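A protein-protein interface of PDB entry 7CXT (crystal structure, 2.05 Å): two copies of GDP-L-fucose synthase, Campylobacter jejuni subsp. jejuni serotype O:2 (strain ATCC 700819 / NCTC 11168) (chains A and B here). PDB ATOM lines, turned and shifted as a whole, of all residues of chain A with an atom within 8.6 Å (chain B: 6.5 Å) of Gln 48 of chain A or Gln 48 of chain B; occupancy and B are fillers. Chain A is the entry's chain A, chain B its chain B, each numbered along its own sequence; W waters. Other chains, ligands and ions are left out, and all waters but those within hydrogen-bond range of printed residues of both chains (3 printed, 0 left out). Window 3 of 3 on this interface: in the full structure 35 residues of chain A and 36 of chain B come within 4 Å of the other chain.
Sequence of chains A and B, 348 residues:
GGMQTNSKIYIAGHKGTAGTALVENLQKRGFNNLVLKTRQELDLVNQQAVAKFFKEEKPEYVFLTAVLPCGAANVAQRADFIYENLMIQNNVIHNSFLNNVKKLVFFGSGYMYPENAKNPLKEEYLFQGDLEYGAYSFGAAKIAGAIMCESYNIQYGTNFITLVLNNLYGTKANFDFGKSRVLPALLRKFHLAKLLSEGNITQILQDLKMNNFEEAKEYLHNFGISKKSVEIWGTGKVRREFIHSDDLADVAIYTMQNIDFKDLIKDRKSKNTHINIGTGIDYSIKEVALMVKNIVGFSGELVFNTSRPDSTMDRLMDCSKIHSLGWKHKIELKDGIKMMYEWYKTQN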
ATOM      1  N   LEU A  42       1.694  33.293   3.285  1.00  0.00           N
ATOM      2  CA  LEU A  42       1.890  32.383   2.156  1.00  0.00           C
ATOM      3  C   LEU A  42       2.388  31.044   2.690  1.00  0.00           C
ATOM      4  O   LEU A  42       3.530  30.930   3.138  1.00  0.00           O
ATOM      5  CB  LEU A  42       2.867  32.978   1.134  1.00  0.00           C
ATOM      6  CG  LEU A  42       3.451  32.051   0.061  1.00  0.00           C
ATOM      7  CD1 LEU A  42       2.358  31.438  -0.819  1.00  0.00           C
ATOM      8  CD2 LEU A  42       4.509  32.782  -0.813  1.00  0.00           C
ATOM      9  N   ASP A  43       1.532  30.030   2.656  1.00  0.00           N
ATOM     10  CA  ASP A  43       1.914  28.683   3.073  1.00  0.00           C
ATOM     11  C   ASP A  43       2.500  27.970   1.856  1.00  0.00           C
ATOM     12  O   ASP A  43       1.759  27.559   0.961  1.00  0.00           O
ATOM     13  CB  ASP A  43       0.708  27.939   3.646  1.00  0.00           C
ATOM     14  CG  ASP A  43       1.032  26.509   4.070  1.00  0.00           C
ATOM     15  OD1 ASP A  43       2.172  26.049   3.884  1.00  0.00           O
ATOM     16  OD2 ASP A  43       0.116  25.835   4.582  1.00  0.00           O
ATOM     17  N   LEU A  44       3.829  27.790   1.842  1.00  0.00           N
ATOM     18  CA  LEU A  44       4.511  27.248   0.678  1.00  0.00           C
ATOM     19  C   LEU A  44       4.170  25.791   0.390  1.00  0.00           C
ATOM     20  O   LEU A  44       4.562  25.288  -0.673  1.00  0.00           O
ATOM     21  CB  LEU A  44       6.022  27.394   0.851  1.00  0.00           C
ATOM     22  CG  LEU A  44       6.471  28.850   0.806  1.00  0.00           C
ATOM     23  CD1 LEU A  44       7.943  28.913   1.193  1.00  0.00           C
ATOM     24  CD2 LEU A  44       6.202  29.457  -0.575  1.00  0.00           C
ATOM     25  N   VAL A  45       3.532  25.085   1.325  1.00  0.00           N
ATOM     26  CA  VAL A  45       3.031  23.742   1.040  1.00  0.00           C
ATOM     27  C   VAL A  45       1.778  23.791   0.167  1.00  0.00           C
ATOM     28  O   VAL A  45       1.435  22.810  -0.509  1.00  0.00           O
ATOM     29  CB  VAL A  45       2.771  23.018   2.375  1.00  0.00           C
ATOM     30  CG1 VAL A  45       1.964  21.689   2.193  1.00  0.00           C
ATOM     31  CG2 VAL A  45       4.091  22.753   3.075  1.00  0.00           C
ATOM     32  N   ASN A  46       1.090  24.921   0.150  1.00  0.00           N
ATOM     33  CA  ASN A  46      -0.172  25.047  -0.565  1.00  0.00           C
ATOM     34  C   ASN A  46       0.107  25.496  -1.995  1.00  0.00           C
ATOM     35  O   ASN A  46       0.510  26.641  -2.229  1.00  0.00           O
ATOM     36  CB  ASN A  46      -1.087  26.030   0.149  1.00  0.00           C
ATOM     37  CG  ASN A  46      -2.464  26.052  -0.448  1.00  0.00           C
ATOM     38  OD1 ASN A  46      -2.715  26.749  -1.423  1.00  0.00           O
ATOM     39  ND2 ASN A  46      -3.362  25.261   0.116  1.00  0.00           N
ATOM     40  N   GLN A  47      -0.119  24.589  -2.948  1.00  0.00           N
ATOM     41  CA  GLN A  47       0.239  24.848  -4.339  1.00  0.00           C
ATOM     42  C   GLN A  47      -0.545  26.021  -4.919  1.00  0.00           C
ATOM     43  O   GLN A  47      -0.006  26.806  -5.706  1.00  0.00           O
ATOM     44  CB  GLN A  47       0.002  23.583  -5.161  1.00  0.00           C
ATOM     45  CG  GLN A  47       0.006  23.756  -6.679  1.00  0.00           C
ATOM     46  CD  GLN A  47      -0.579  22.524  -7.362  1.00  0.00           C
ATOM     47  OE1 GLN A  47      -1.750  22.201  -7.175  1.00  0.00           O
ATOM     48  NE2 GLN A  47       0.250  21.808  -8.113  1.00  0.00           N
ATOM     49  N   GLN A  48      -1.819  26.164  -4.533  1.00  0.00           N
ATOM     50  CA  GLN A  48      -2.641  27.233  -5.094  1.00  0.00           C
ATOM     51  C   GLN A  48      -2.130  28.589  -4.658  1.00  0.00           C
ATOM     52  O   GLN A  48      -2.051  29.521  -5.464  1.00  0.00           O
ATOM     53  CB  GLN A  48      -4.109  27.069  -4.659  1.00  0.00           C
ATOM     54  CG  GLN A  48      -5.058  28.195  -5.079  1.00  0.00           C
ATOM     55  CD  GLN A  48      -6.456  28.086  -4.428  1.00  0.00           C
ATOM     56  OE1 GLN A  48      -6.661  27.326  -3.481  1.00  0.00           O
ATOM     57  NE2 GLN A  48      -7.411  28.849  -4.944  1.00  0.00           N
ATOM     58  N   ALA A  49      -1.791  28.717  -3.374  1.00  0.00           N
ATOM     59  CA  ALA A  49      -1.226  29.960  -2.887  1.00  0.00           C
ATOM     60  C   ALA A  49       0.115  30.254  -3.556  1.00  0.00           C
ATOM     61  O   ALA A  49       0.398  31.403  -3.899  1.00  0.00           O
ATOM     62  CB  ALA A  49      -1.091  29.892  -1.365  1.00  0.00           C
ATOM     63  N   VAL A  50       0.941  29.229  -3.790  1.00  0.00           N
ATOM     64  CA  VAL A  50       2.240  29.501  -4.403  1.00  0.00           C
ATOM     65  C   VAL A  50       2.059  29.913  -5.856  1.00  0.00           C
ATOM     66  O   VAL A  50       2.655  30.895  -6.316  1.00  0.00           O
ATOM     67  CB  VAL A  50       3.170  28.284  -4.251  1.00  0.00           C
ATOM     68  CG1 VAL A  50       4.495  28.490  -5.022  1.00  0.00           C
ATOM     69  CG2 VAL A  50       3.448  28.032  -2.780  1.00  0.00           C
ATOM     70  N   ALA A  51       1.189  29.214  -6.589  1.00  0.00           N
ATOM     71  CA  ALA A  51       0.941  29.593  -7.977  1.00  0.00           C
ATOM     72  C   ALA A  51       0.379  31.005  -8.073  1.00  0.00           C
ATOM     73  O   ALA A  51       0.750  31.761  -8.979  1.00  0.00           O
ATOM     74  CB  ALA A  51      -0.014  28.601  -8.637  1.00  0.00           C
ATOM     75  N   LYS A  52      -0.494  31.394  -7.133  1.00  0.00           N
ATOM     76  CA  LYS A  52      -1.030  32.751  -7.159  1.00  0.00           C
ATOM     77  C   LYS A  52       0.057  33.779  -6.875  1.00  0.00           C
ATOM     78  O   LYS A  52       0.090  34.842  -7.505  1.00  0.00           O
ATOM     79  CB  LYS A  52      -2.177  32.890  -6.153  1.00  0.00           C
ATOM     80  CG  LYS A  52      -3.580  32.816  -6.751  1.00  0.00           C
ATOM     81  CD  LYS A  52      -4.167  31.418  -6.753  1.00  0.00           C
ATOM     82  CE  LYS A  52      -3.685  30.601  -7.952  1.00  0.00           C
ATOM     83  NZ  LYS A  52      -3.961  29.147  -7.804  1.00  0.00           N
ATOM     84  N   PHE A  53       0.961  33.472  -5.941  1.00  0.00           N
ATOM     85  CA  PHE A  53       2.041  34.402  -5.610  1.00  0.00           C
ATOM     86  C   PHE A  53       2.955  34.649  -6.808  1.00  0.00           C
ATOM     87  O   PHE A  53       3.334  35.793  -7.093  1.00  0.00           O
ATOM     88  CB  PHE A  53       2.863  33.854  -4.437  1.00  0.00           C
ATOM     89  CG  PHE A  53       4.203  34.551  -4.265  1.00  0.00           C
ATOM     90  CD1 PHE A  53       4.292  35.750  -3.564  1.00  0.00           C
ATOM     91  CD2 PHE A  53       5.362  34.022  -4.839  1.00  0.00           C
ATOM     92  CE1 PHE A  53       5.505  36.398  -3.409  1.00  0.00           C
ATOM     93  CE2 PHE A  53       6.589  34.680  -4.701  1.00  0.00           C
ATOM     94  CZ  PHE A  53       6.661  35.863  -3.984  1.00  0.00           C
ATOM     95  N   PHE A  54       3.355  33.579  -7.502  1.00  0.00           N
ATOM     96  CA  PHE A  54       4.264  33.755  -8.628  1.00  0.00           C
ATOM     97  C   PHE A  54       3.592  34.465  -9.789  1.00  0.00           C
ATOM     98  O   PHE A  54       4.244  35.223 -10.508  1.00  0.00           O
ATOM     99  CB  PHE A  54       4.823  32.403  -9.084  1.00  0.00           C
ATOM    100  CG  PHE A  54       6.041  31.982  -8.325  1.00  0.00           C
ATOM    101  CD1 PHE A  54       5.926  31.270  -7.145  1.00  0.00           C
ATOM    102  CD2 PHE A  54       7.304  32.344  -8.775  1.00  0.00           C
ATOM    103  CE1 PHE A  54       7.060  30.902  -6.424  1.00  0.00           C
ATOM    104  CE2 PHE A  54       8.439  31.987  -8.064  1.00  0.00           C
ATOM    105  CZ  PHE A  54       8.322  31.269  -6.890  1.00  0.00           C
ATOM    106  N   LYS A  55       2.288  34.204 -10.015  1.00  0.00           N
ATOM    107  CA  LYS A  55       1.554  34.914 -11.064  1.00  0.00           C
ATOM    108  C   LYS A  55       1.427  36.402 -10.764  1.00  0.00           C
ATOM    109  O   LYS A  55       1.451  37.226 -11.687  1.00  0.00           O
ATOM    110  CB  LYS A  55       0.149  34.305 -11.244  1.00  0.00           C
ATOM    111  CG  LYS A  55       0.099  33.061 -12.141  1.00  0.00           C
ATOM    112  CD  LYS A  55      -1.333  32.464 -12.159  1.00  0.00           C
ATOM    113  CE  LYS A  55      -1.367  31.091 -12.823  1.00  0.00           C
ATOM    114  NZ  LYS A  55      -2.728  30.462 -12.771  1.00  0.00           N
ATOM    115  N   MET A  87       6.748  19.266  -0.979  1.00  0.00           N
ATOM    116  CA  MET A  87       5.714  20.176  -1.480  1.00  0.00           C
ATOM    117  C   MET A  87       6.257  21.593  -1.643  1.00  0.00           C
ATOM    118  O   MET A  87       5.992  22.258  -2.655  1.00  0.00           O
ATOM    119  CB  MET A  87       4.504  20.187  -0.532  1.00  0.00           C
ATOM    120  CG  MET A  87       3.639  18.927  -0.563  1.00  0.00           C
ATOM    121  SD  MET A  87       2.977  18.499  -2.184  1.00  0.00           S
ATOM    122  CE  MET A  87       2.070  19.983  -2.610  1.00  0.00           C
ATOM    123  N   ASN A  91       6.391  23.046  -5.305  1.00  0.00           N
ATOM    124  CA  ASN A  91       5.581  24.234  -5.558  1.00  0.00           C
ATOM    125  C   ASN A  91       6.441  25.394  -6.032  1.00  0.00           C
ATOM    126  O   ASN A  91       6.129  26.038  -7.036  1.00  0.00           O
ATOM    127  CB  ASN A  91       4.821  24.658  -4.296  1.00  0.00           C
ATOM    128  CG  ASN A  91       3.639  23.741  -3.970  1.00  0.00           C
ATOM    129  OD1 ASN A  91       3.118  23.035  -4.838  1.00  0.00           O
ATOM    130  ND2 ASN A  91       3.216  23.754  -2.710  1.00  0.00           N
ATOM    131  N   ASN A  95       6.578  26.415 -10.150  1.00  0.00           N
ATOM    132  CA  ASN A  95       5.968  27.697 -10.437  1.00  0.00           C
ATOM    133  C   ASN A  95       6.995  28.759 -10.795  1.00  0.00           C
ATOM    134  O   ASN A  95       6.659  29.689 -11.530  1.00  0.00           O
ATOM    135  CB  ASN A  95       5.077  28.107  -9.260  1.00  0.00           C
ATOM    136  CG  ASN A  95       3.777  27.342  -9.266  1.00  0.00           C
ATOM    137  OD1 ASN A  95       2.887  27.657 -10.043  1.00  0.00           O
ATOM    138  ND2 ASN A  95       3.686  26.291  -8.452  1.00  0.00           N
ATOM    139  N   VAL B  45      -2.325  16.130 -10.376  1.00  0.00           N
ATOM    140  CA  VAL B  45      -1.243  17.063 -10.034  1.00  0.00           C
ATOM    141  C   VAL B  45      -1.759  18.294  -9.276  1.00  0.00           C
ATOM    142  O   VAL B  45      -1.012  18.924  -8.515  1.00  0.00           O
ATOM    143  CB  VAL B  45      -0.486  17.459 -11.318  1.00  0.00           C
ATOM    144  CG1 VAL B  45       0.548  18.556 -11.045  1.00  0.00           C
ATOM    145  CG2 VAL B  45       0.205  16.226 -11.921  1.00  0.00           C
ATOM    146  N   ASN B  46      -3.035  18.635  -9.430  1.00  0.00           N
ATOM    147  CA  ASN B  46      -3.603  19.797  -8.766  1.00  0.00           C
ATOM    148  C   ASN B  46      -3.991  19.422  -7.340  1.00  0.00           C
ATOM    149  O   ASN B  46      -4.945  18.665  -7.129  1.00  0.00           O
ATOM    150  CB  ASN B  46      -4.798  20.308  -9.557  1.00  0.00           C
ATOM    151  CG  ASN B  46      -5.349  21.574  -8.991  1.00  0.00           C
ATOM    152  OD1 ASN B  46      -6.142  21.546  -8.056  1.00  0.00           O
ATOM    153  ND2 ASN B  46      -4.919  22.707  -9.537  1.00  0.00           N
ATOM    154  N   GLN B  47      -3.239  19.943  -6.362  1.00  0.00           N
ATOM    155  CA  GLN B  47      -3.482  19.593  -4.966  1.00  0.00           C
ATOM    156  C   GLN B  47      -4.886  20.014  -4.522  1.00  0.00           C
ATOM    157  O   GLN B  47      -5.552  19.288  -3.778  1.00  0.00           O
ATOM    158  CB  GLN B  47      -2.411  20.248  -4.073  1.00  0.00           C
ATOM    159  CG  GLN B  47      -2.693  20.208  -2.558  1.00  0.00           C
ATOM    160  CD  GLN B  47      -1.788  21.142  -1.753  1.00  0.00           C
ATOM    161  OE1 GLN B  47      -1.716  22.341  -2.030  1.00  0.00           O
ATOM    162  NE2 GLN B  47      -1.070  20.589  -0.774  1.00  0.00           N
ATOM    163  N   GLN B  48      -5.364  21.167  -4.996  1.00  0.00           N
ATOM    164  CA  GLN B  48      -6.662  21.671  -4.544  1.00  0.00           C
ATOM    165  C   GLN B  48      -7.777  20.719  -4.950  1.00  0.00           C
ATOM    166  O   GLN B  48      -8.642  20.356  -4.139  1.00  0.00           O
ATOM    167  CB  GLN B  48      -6.911  23.065  -5.125  1.00  0.00           C
ATOM    168  CG  GLN B  48      -8.319  23.616  -4.874  1.00  0.00           C
ATOM    169  CD  GLN B  48      -8.521  25.003  -5.492  1.00  0.00           C
ATOM    170  OE1 GLN B  48      -7.876  25.359  -6.478  1.00  0.00           O
ATOM    171  NE2 GLN B  48      -9.422  25.780  -4.916  1.00  0.00           N
ATOM    172  N   ALA B  49      -7.741  20.275  -6.203  1.00  0.00           N
ATOM    173  CA  ALA B  49      -8.739  19.339  -6.704  1.00  0.00           C
ATOM    174  C   ALA B  49      -8.680  18.000  -5.979  1.00  0.00           C
ATOM    175  O   ALA B  49      -9.725  17.387  -5.717  1.00  0.00           O
ATOM    176  CB  ALA B  49      -8.538  19.154  -8.203  1.00  0.00           C
ATOM    177  N   VAL B  50      -7.471  17.517  -5.658  1.00  0.00           N
ATOM    178  CA  VAL B  50      -7.362  16.213  -5.005  1.00  0.00           C
ATOM    179  C   VAL B  50      -7.862  16.293  -3.566  1.00  0.00           C
ATOM    180  O   VAL B  50      -8.567  15.396  -3.085  1.00  0.00           O
ATOM    181  CB  VAL B  50      -5.919  15.677  -5.076  1.00  0.00           C
ATOM    182  CG1 VAL B  50      -5.783  14.372  -4.284  1.00  0.00           C
ATOM    183  CG2 VAL B  50      -5.497  15.456  -6.542  1.00  0.00           C
ATOM    184  N   ALA B  51      -7.504  17.364  -2.856  1.00  0.00           N
ATOM    185  CA  ALA B  51      -7.966  17.525  -1.483  1.00  0.00           C
ATOM    186  C   ALA B  51      -9.482  17.641  -1.440  1.00  0.00           C
ATOM    187  O   ALA B  51     -10.136  17.080  -0.553  1.00  0.00           O
ATOM    188  CB  ALA B  51      -7.315  18.765  -0.853  1.00  0.00           C
ATOM    189  N   LYS B  52     -10.068  18.306  -2.436  1.00  0.00           N
ATOM    190  CA  LYS B  52     -11.523  18.369  -2.491  1.00  0.00           C
ATOM    191  C   LYS B  52     -12.128  16.989  -2.754  1.00  0.00           C
ATOM    192  O   LYS B  52     -13.138  16.621  -2.142  1.00  0.00           O
ATOM    193  CB  LYS B  52     -11.954  19.369  -3.558  1.00  0.00           C
ATOM    194  CG  LYS B  52     -13.463  19.516  -3.694  1.00  0.00           C
ATOM    195  CD  LYS B  52     -13.824  20.505  -4.782  1.00  0.00           C
ATOM    196  CE  LYS B  52     -15.350  20.637  -4.877  1.00  0.00           C
ATOM    197  NZ  LYS B  52     -15.782  21.451  -6.036  1.00  0.00           N
ATOM    198  N   PHE B  53     -11.499  16.189  -3.618  1.00  0.00           N
ATOM    199  CA  PHE B  53     -12.080  14.885  -3.958  1.00  0.00           C
ATOM    200  C   PHE B  53     -12.116  13.950  -2.753  1.00  0.00           C
ATOM    201  O   PHE B  53     -13.138  13.311  -2.493  1.00  0.00           O
ATOM    202  CB  PHE B  53     -11.308  14.257  -5.122  1.00  0.00           C
ATOM    203  CG  PHE B  53     -11.532  12.781  -5.295  1.00  0.00           C
ATOM    204  CD1 PHE B  53     -12.548  12.317  -6.108  1.00  0.00           C
ATOM    205  CD2 PHE B  53     -10.701  11.853  -4.671  1.00  0.00           C
ATOM    206  CE1 PHE B  53     -12.754  10.941  -6.278  1.00  0.00           C
ATOM    207  CE2 PHE B  53     -10.897  10.490  -4.835  1.00  0.00           C
ATOM    208  CZ  PHE B  53     -11.927  10.036  -5.643  1.00  0.00           C
ATOM    209  N   ASN B  91      -0.050  14.273  -3.511  1.00  0.00           N
ATOM    210  CA  ASN B  91      -1.444  14.686  -3.323  1.00  0.00           C
ATOM    211  C   ASN B  91      -2.314  13.516  -2.868  1.00  0.00           C
ATOM    212  O   ASN B  91      -3.101  13.641  -1.919  1.00  0.00           O
ATOM    213  CB  ASN B  91      -1.992  15.304  -4.618  1.00  0.00           C
ATOM    214  CG  ASN B  91      -1.393  16.700  -4.906  1.00  0.00           C
ATOM    215  OD1 ASN B  91      -0.895  17.363  -4.006  1.00  0.00           O
ATOM    216  ND2 ASN B  91      -1.459  17.139  -6.166  1.00  0.00           N
HETATM  217  O   HOH W   1      -3.475  23.882  -3.551  1.00  0.00           O
HETATM  218  O   HOH W   2      -3.759  23.266  -6.014  1.00  0.00           O
HETATM  219  O   HOH W   3      -8.683  26.895  -1.877  1.00  0.00           O
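The backbone carbonyl oxygen of Val 45 of chain A sits at hydrogen-bond distance from the side-chain amide nitrogen of Gln 47 of chain B.
The side-chain amide nitrogen (NE2) of Gln 47 of chain A lies within hydrogen-bond range of the backbone carbonyl oxygen (O) of Val 45 of chain B (3.2 Å).
N of Gln 47 of chain B is in hydrogen-bond range of OE1 of Gln 47 of chain A, at 2.8 Å.
The side-chain amide nitrogen (NE2) of Gln 48 of chain B is in hydrogen-bond range of the side-chain amide oxygen (OE1) of Gln 48 of chain A (3.5 Å).
N of Val 45 of chain A is in hydrogen-bond range of OD1 of Asp 43 of chain A.
The side-chain amide nitrogen of Asn 91 of chain A is in hydrogen-bond range of the backbone carbonyl oxygen of Val 45 of chain A, 3.0 Å away.
The side-chain amide oxygen (OD1) of Asn 46 of chain A sits close to the backbone NH (N) of Gln 48 of chain A (3.3 Å).
ND2 of Asn 91 of chain B is in hydrogen-bond range of O of Val 45 of chain B, 3.0 Å away.
The side-chain amide oxygen (OD1) of Asn 46 of chain B sits at hydrogen-bond distance from the backbone NH (N) of Ala 49 of chain B, 2.8 Å away.
The backbone NH of Gln 47 of chain B lies close to the side-chain amide nitrogen of Asn 91 of chain B, 3.3 Å away.
Among the printed residues, merely in contact across the chains: Gln 47 of chain A with Asn 46 of chain B, Asn 46 of chain A with Gln 47 of chain B and Met 87 of chain A with Gln 47 of chain B.
Gln 48 of chain A touches just one residue of chain B: Gln 48 (3.5 Å).
Of the printed residues of chain A, Gln 48 of chain B touches Gln 48.
Printed residues of chain B within 4 Å of Val 45 of chain A: Gln 47.
Printed residues of chain A within 4 Å of Asn 46 of chain B: Gln 47.
Printed residues of chain A within 4 Å of Val 45 of chain B: Gln 47.
Printed residues of chain A within 4 Å of Gln 47 of chain B: Val 45 (3.4 Å), Asn 46 (3.4 Å), Gln 47 (2.8 Å) and Met 87 (3.7 Å).
Val 50 of chain B touches none of the printed residues of chain A.
The nearest residue of chain B that does not touch Gln 48 of chain A is Gln 47 of chain B (4.6 Å).
The nearest printed residue of chain A that does not touch Gln 47 of chain B is Gln 48 of chain A (4.6 Å).
Printed residues of chain A that touch a printed residue of chain B: Val 45, Asn 46, Gln 47, Gln 48 and Met 87.
Hydrophobic or aromatic side chains of chain A that line the printed part of chain B: Met 87.
Of the 10 printed residues of chain B, 4 touch a printed residue of chain A.
Among the printed residues, no Asp or Glu carboxylate lies within 4 Å of a Lys or Arg side-chain nitrogen of the other chain.
Val 45 of chain A touches Gln 47 of chain B, and with the chains exchanged Gln 47 of chain A touches Val 45 of chain B.
Asn 46 of chain A touches Gln 47 of chain B, and with the chains exchanged Gln 47 of chain A touches Asn 46 of chain B.
Gln 47 of chain B touches its own counterpart, Gln 47 of chain A.
Gln 48 of chain A touches its own counterpart, Gln 48 of chain B.
Water W2 lies within hydrogen-bond range of the side-chain amide oxygen of Gln 47 of chain A, the backbone NH of Gln 48 of chain B and the backbone NH of Gln 47 of chain B.
Water W3 lies within hydrogen-bond range of OE1 of Gln 48 of chain A (2.6 Å) and NE2 of Gln 48 of chain B (3.3 Å).
Water W1 lies within hydrogen-bond range of OE1 of Gln 47 of chain B, N of Gln 48 of chain A and N of Gln 47 of chain A.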
